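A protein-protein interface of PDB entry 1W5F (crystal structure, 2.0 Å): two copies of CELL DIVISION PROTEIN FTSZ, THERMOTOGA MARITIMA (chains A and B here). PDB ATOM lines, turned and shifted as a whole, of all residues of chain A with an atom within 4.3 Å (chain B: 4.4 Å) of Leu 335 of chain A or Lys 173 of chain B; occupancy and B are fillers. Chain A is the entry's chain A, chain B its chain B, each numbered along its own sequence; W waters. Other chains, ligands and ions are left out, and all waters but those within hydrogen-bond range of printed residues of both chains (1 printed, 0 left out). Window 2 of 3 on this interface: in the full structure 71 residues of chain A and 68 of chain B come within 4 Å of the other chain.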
ATOM      1  N   ALA A 235     -10.901  19.288 -13.765  1.00  0.00           N
ATOM      2  CA  ALA A 235     -10.402  18.465 -12.673  1.00  0.00           C
ATOM      3  C   ALA A 235      -9.061  19.018 -12.221  1.00  0.00           C
ATOM      4  O   ALA A 235      -8.239  19.418 -13.044  1.00  0.00           O
ATOM      5  CB  ALA A 235     -10.249  17.016 -13.138  1.00  0.00           C
ATOM      6  N   GLU A 263      -3.475  11.026  -7.152  1.00  0.00           N
ATOM      7  CA  GLU A 263      -3.696   9.807  -7.923  1.00  0.00           C
ATOM      8  C   GLU A 263      -3.151   9.863  -9.343  1.00  0.00           C
ATOM      9  O   GLU A 263      -2.927   8.824  -9.966  1.00  0.00           O
ATOM     10  CB  GLU A 263      -5.191   9.504  -7.981  1.00  0.00           C
ATOM     11  CG  GLU A 263      -5.834   9.303  -6.628  1.00  0.00           C
ATOM     12  CD  GLU A 263      -7.315   9.017  -6.735  1.00  0.00           C
ATOM     13  OE1 GLU A 263      -8.073   9.933  -7.120  1.00  0.00           O
ATOM     14  OE2 GLU A 263      -7.716   7.872  -6.439  1.00  0.00           O
ATOM     15  N   GLU A 331      -8.631  14.239 -18.172  1.00  0.00           N
ATOM     16  CA  GLU A 331      -9.170  14.398 -16.821  1.00  0.00           C
ATOM     17  C   GLU A 331      -9.710  13.097 -16.238  1.00  0.00           C
ATOM     18  O   GLU A 331      -9.693  12.900 -15.023  1.00  0.00           O
ATOM     19  CB  GLU A 331     -10.286  15.446 -16.806  1.00  0.00           C
ATOM     20  CG  GLU A 331      -9.866  16.834 -17.250  1.00  0.00           C
ATOM     21  CD  GLU A 331     -10.975  17.853 -17.074  1.00  0.00           C
ATOM     22  OE1 GLU A 331     -10.825  18.991 -17.569  1.00  0.00           O
ATOM     23  OE2 GLU A 331     -11.995  17.516 -16.436  1.00  0.00           O
ATOM     24  N   ASP A 332     -10.195  12.216 -17.105  1.00  0.00           N
ATOM     25  CA  ASP A 332     -10.745  10.943 -16.661  1.00  0.00           C
ATOM     26  C   ASP A 332      -9.769  10.196 -15.765  1.00  0.00           C
ATOM     27  O   ASP A 332     -10.175   9.522 -14.819  1.00  0.00           O
ATOM     28  CB  ASP A 332     -11.108  10.081 -17.871  1.00  0.00           C
ATOM     29  CG  ASP A 332     -12.190  10.711 -18.728  1.00  0.00           C
ATOM     30  OD1 ASP A 332     -12.521  10.138 -19.787  1.00  0.00           O
ATOM     31  OD2 ASP A 332     -12.709  11.778 -18.340  1.00  0.00           O
ATOM     32  N   LYS A 333      -8.480  10.326 -16.061  1.00  0.00           N
ATOM     33  CA  LYS A 333      -7.439   9.660 -15.284  1.00  0.00           C
ATOM     34  C   LYS A 333      -7.478  10.100 -13.821  1.00  0.00           C
ATOM     35  O   LYS A 333      -7.164   9.323 -12.919  1.00  0.00           O
ATOM     36  CB  LYS A 333      -6.064   9.975 -15.878  1.00  0.00           C
ATOM     37  CG  LYS A 333      -5.196   8.752 -16.146  1.00  0.00           C
ATOM     38  CD  LYS A 333      -5.793   7.874 -17.234  1.00  0.00           C
ATOM     39  CE  LYS A 333      -4.894   6.690 -17.542  1.00  0.00           C
ATOM     40  NZ  LYS A 333      -5.431   5.863 -18.657  1.00  0.00           N
ATOM     41  N   ILE A 334      -7.865  11.352 -13.596  1.00  0.00           N
ATOM     42  CA  ILE A 334      -7.950  11.907 -12.249  1.00  0.00           C
ATOM     43  C   ILE A 334      -9.298  11.621 -11.603  1.00  0.00           C
ATOM     44  O   ILE A 334      -9.369  11.131 -10.478  1.00  0.00           O
ATOM     45  CB  ILE A 334      -7.749  13.437 -12.259  1.00  0.00           C
ATOM     46  CG1 ILE A 334      -6.350  13.772 -12.773  1.00  0.00           C
ATOM     47  CG2 ILE A 334      -7.957  14.003 -10.855  1.00  0.00           C
ATOM     48  CD1 ILE A 334      -6.072  15.247 -12.838  1.00  0.00           C
ATOM     49  N   LEU A 335     -10.371  11.931 -12.320  1.00  0.00           N
ATOM     50  CA  LEU A 335     -11.709  11.716 -11.794  1.00  0.00           C
ATOM     51  C   LEU A 335     -12.088  10.250 -11.599  1.00  0.00           C
ATOM     52  O   LEU A 335     -12.783   9.913 -10.639  1.00  0.00           O
ATOM     53  CB  LEU A 335     -12.737  12.393 -12.697  1.00  0.00           C
ATOM     54  CG  LEU A 335     -12.618  13.913 -12.806  1.00  0.00           C
ATOM     55  CD1 LEU A 335     -13.759  14.434 -13.660  1.00  0.00           C
ATOM     56  CD2 LEU A 335     -12.652  14.546 -11.416  1.00  0.00           C
ATOM     57  N   PHE A 336     -11.639   9.373 -12.496  1.00  0.00           N
ATOM     58  CA  PHE A 336     -11.988   7.960 -12.374  1.00  0.00           C
ATOM     59  C   PHE A 336     -10.792   7.020 -12.514  1.00  0.00           C
ATOM     60  O   PHE A 336     -10.269   6.585 -11.466  1.00  0.00           O
ATOM     61  CB  PHE A 336     -13.050   7.605 -13.419  1.00  0.00           C
ATOM     62  CG  PHE A 336     -14.090   8.676 -13.612  1.00  0.00           C
ATOM     63  CD1 PHE A 336     -13.993   9.575 -14.671  1.00  0.00           C
ATOM     64  CD2 PHE A 336     -15.150   8.805 -12.721  1.00  0.00           C
ATOM     65  CE1 PHE A 336     -14.939  10.591 -14.839  1.00  0.00           C
ATOM     66  CE2 PHE A 336     -16.100   9.816 -12.881  1.00  0.00           C
ATOM     67  CZ  PHE A 336     -15.993  10.711 -13.942  1.00  0.00           C
ATOM     68  N   VAL B 142     -14.948  17.602  -3.175  1.00  0.00           N
ATOM     69  CA  VAL B 142     -15.788  16.505  -2.716  1.00  0.00           C
ATOM     70  C   VAL B 142     -15.013  15.200  -2.610  1.00  0.00           C
ATOM     71  O   VAL B 142     -13.952  15.048  -3.209  1.00  0.00           O
ATOM     72  CB  VAL B 142     -16.970  16.298  -3.683  1.00  0.00           C
ATOM     73  CG1 VAL B 142     -17.733  17.613  -3.869  1.00  0.00           C
ATOM     74  CG2 VAL B 142     -16.457  15.799  -5.030  1.00  0.00           C
ATOM     75  N   THR B 144     -14.978  10.721  -2.585  1.00  0.00           N
ATOM     76  CA  THR B 144     -15.607   9.503  -3.090  1.00  0.00           C
ATOM     77  C   THR B 144     -15.543   8.572  -1.868  1.00  0.00           C
ATOM     78  O   THR B 144     -14.620   8.673  -1.054  1.00  0.00           O
ATOM     79  CB  THR B 144     -14.844   8.903  -4.299  1.00  0.00           C
ATOM     80  OG1 THR B 144     -13.433   8.937  -4.055  1.00  0.00           O
ATOM     81  CG2 THR B 144     -15.159   9.692  -5.561  1.00  0.00           C
ATOM     82  N   LEU B 161     -20.130  12.617 -10.025  1.00  0.00           N
ATOM     83  CA  LEU B 161     -18.967  13.363 -10.516  1.00  0.00           C
ATOM     84  C   LEU B 161     -19.097  13.742 -11.988  1.00  0.00           C
ATOM     85  O   LEU B 161     -18.625  14.802 -12.409  1.00  0.00           O
ATOM     86  CB  LEU B 161     -17.682  12.550 -10.310  1.00  0.00           C
ATOM     87  CG  LEU B 161     -17.155  12.427  -8.874  1.00  0.00           C
ATOM     88  CD1 LEU B 161     -15.978  11.457  -8.846  1.00  0.00           C
ATOM     89  CD2 LEU B 161     -16.724  13.803  -8.352  1.00  0.00           C
ATOM     90  N   ARG B 165     -18.899  17.700 -12.855  1.00  0.00           N
ATOM     91  CA  ARG B 165     -17.859  18.120 -13.782  1.00  0.00           C
ATOM     92  C   ARG B 165     -18.322  19.146 -14.816  1.00  0.00           C
ATOM     93  O   ARG B 165     -17.585  20.066 -15.162  1.00  0.00           O
ATOM     94  CB  ARG B 165     -17.316  16.875 -14.482  1.00  0.00           C
ATOM     95  CG  ARG B 165     -16.304  17.110 -15.576  1.00  0.00           C
ATOM     96  CD  ARG B 165     -15.966  15.766 -16.205  1.00  0.00           C
ATOM     97  NE  ARG B 165     -14.928  15.852 -17.225  1.00  0.00           N
ATOM     98  CZ  ARG B 165     -14.419  14.796 -17.850  1.00  0.00           C
ATOM     99  NH1 ARG B 165     -14.857  13.578 -17.555  1.00  0.00           N
ATOM    100  NH2 ARG B 165     -13.472  14.953 -18.766  1.00  0.00           N
ATOM    101  N   LEU B 171     -12.709  21.293 -10.110  1.00  0.00           N
ATOM    102  CA  LEU B 171     -13.233  20.165  -9.351  1.00  0.00           C
ATOM    103  C   LEU B 171     -12.086  19.415  -8.677  1.00  0.00           C
ATOM    104  O   LEU B 171     -11.258  18.800  -9.350  1.00  0.00           O
ATOM    105  CB  LEU B 171     -14.003  19.211 -10.278  1.00  0.00           C
ATOM    106  CG  LEU B 171     -15.012  18.250  -9.634  1.00  0.00           C
ATOM    107  CD1 LEU B 171     -15.767  17.507 -10.733  1.00  0.00           C
ATOM    108  CD2 LEU B 171     -14.305  17.264  -8.716  1.00  0.00           C
ATOM    109  N   ILE B 172     -12.037  19.481  -7.350  1.00  0.00           N
ATOM    110  CA  ILE B 172     -11.010  18.787  -6.586  1.00  0.00           C
ATOM    111  C   ILE B 172     -11.672  17.563  -5.953  1.00  0.00           C
ATOM    112  O   ILE B 172     -12.530  17.694  -5.077  1.00  0.00           O
ATOM    113  CB  ILE B 172     -10.428  19.694  -5.477  1.00  0.00           C
ATOM    114  CG1 ILE B 172      -9.715  20.890  -6.120  1.00  0.00           C
ATOM    115  CG2 ILE B 172      -9.461  18.889  -4.593  1.00  0.00           C
ATOM    116  CD1 ILE B 172      -9.514  22.070  -5.187  1.00  0.00           C
ATOM    117  N   LYS B 173     -11.286  16.376  -6.413  1.00  0.00           N
ATOM    118  CA  LYS B 173     -11.862  15.144  -5.894  1.00  0.00           C
ATOM    119  C   LYS B 173     -10.899  14.474  -4.928  1.00  0.00           C
ATOM    120  O   LYS B 173      -9.747  14.203  -5.270  1.00  0.00           O
ATOM    121  CB  LYS B 173     -12.178  14.178  -7.041  1.00  0.00           C
ATOM    122  CG  LYS B 173     -12.926  12.922  -6.600  1.00  0.00           C
ATOM    123  CD  LYS B 173     -12.508  11.704  -7.406  1.00  0.00           C
ATOM    124  CE  LYS B 173     -11.098  11.263  -7.033  1.00  0.00           C
ATOM    125  NZ  LYS B 173     -10.652  10.098  -7.851  1.00  0.00           N
ATOM    126  N   ILE B 174     -11.375  14.212  -3.718  1.00  0.00           N
ATOM    127  CA  ILE B 174     -10.558  13.566  -2.707  1.00  0.00           C
ATOM    128  C   ILE B 174     -11.010  12.124  -2.521  1.00  0.00           C
ATOM    129  O   ILE B 174     -12.147  11.861  -2.125  1.00  0.00           O
ATOM    130  CB  ILE B 174     -10.655  14.309  -1.358  1.00  0.00           C
ATOM    131  CG1 ILE B 174     -10.038  15.706  -1.490  1.00  0.00           C
ATOM    132  CG2 ILE B 174      -9.947  13.512  -0.273  1.00  0.00           C
ATOM    133  CD1 ILE B 174     -10.272  16.586  -0.293  1.00  0.00           C
ATOM    134  N   SER B 175     -10.116  11.190  -2.823  1.00  0.00           N
ATOM    135  CA  SER B 175     -10.413   9.769  -2.681  1.00  0.00           C
ATOM    136  C   SER B 175     -10.247   9.333  -1.235  1.00  0.00           C
ATOM    137  O   SER B 175      -9.137   9.367  -0.696  1.00  0.00           O
ATOM    138  CB  SER B 175      -9.472   8.946  -3.558  1.00  0.00           C
ATOM    139  OG  SER B 175      -9.525   7.577  -3.198  1.00  0.00           O
HETATM  140  O   HOH W   1     -14.074  19.188 -16.741  1.00  0.00           O
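Of the 8 printed residues of chain A, 6 touch a printed residue of chain B.
Hydrophobic or aromatic side chains of chain A within 4 Å of the printed part of chain B: Leu 335.
Of the 9 printed residues of chain B, 5 touch a printed residue of chain A.
Among the printed residues, 9 pairs touch across the chains.
Among the printed residues, Asp or Glu carboxylates within 4 Å of a Lys or Arg side-chain nitrogen of the other chain: Glu 263 of chain A with Lys 173 of chain B (2.7 Å), Glu 331 of chain A with Arg 165 of chain B (3.5 Å) and Asp 332 of chain A with Arg 165 of chain B (2.9 Å).
Leu 335 of chain A touches just these residues of chain B: Leu 161 (3.98 Å), Arg 165 (3.6 Å) and Lys 173 (3.5 Å).
Lys 173 of chain B touches just these residues of chain A: Glu 263 (2.7 Å), Ile 334 (3.1 Å) and Leu 335 (3.5 Å).
Of the printed residues of chain B, Ala 235 of chain A touches Leu 171.
Of the printed residues of chain A, Arg 165 of chain B touches Glu 331, Asp 332 and Leu 335.
Phe 336 of chain A touches none of the printed residues of chain B.
The nearest printed residue of chain A that does not touch Lys 173 of chain B is Phe 336 of chain A (4.8 Å).
The nearest printed residue of chain A that does not touch Leu 171 of chain B is Leu 335 of chain A (4.2 Å).
No position is printed for both chains.
Of the 9 pairs that touch across the chains among the printed residues, none has its exchanged pair printed and touching as well.
The side-chain carboxylate (OD2) of Asp 332 of chain A lies within salt-bridge range of the guanidinium group (NH1) of Arg 165 of chain B (2.9 Å).
The backbone carbonyl oxygen of Ile 334 of chain A lies within hydrogen-bond range of the side-chain amino group of Lys 173 of chain B (3.1 Å).
The guanidinium group (NE) of Arg 165 of chain B lies within salt-bridge range of the side-chain carboxylate (OE2) of Glu 331 of chain A (3.5 Å).
OE1 of Glu 263 of chain A lies within salt-bridge range of NZ of Lys 173 of chain B (2.7 Å).
Leu 171 of chain B touches Ala 235 of chain A.
Ser 175 of chain B touches Glu 263 of chain A (CB to OE2, 3.5 Å).
Leu 335 of chain A touches Leu 161 of chain B (O to CD1, 3.98 Å).
Arg 165 of chain B touches Leu 335 of chain A.
NZ of Lys 173 of chain B touches O of Leu 335 of chain A (3.5 Å).
N of Ala 235 of chain A sits at hydrogen-bond distance from OE2 of Glu 331 of chain A, 3.4 Å away.
Water W1 bridges the side-chain carboxylate of Glu 331 of chain A (2.7 Å) and the guanidinium group of Arg 165 of chain B (3.5 Å).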
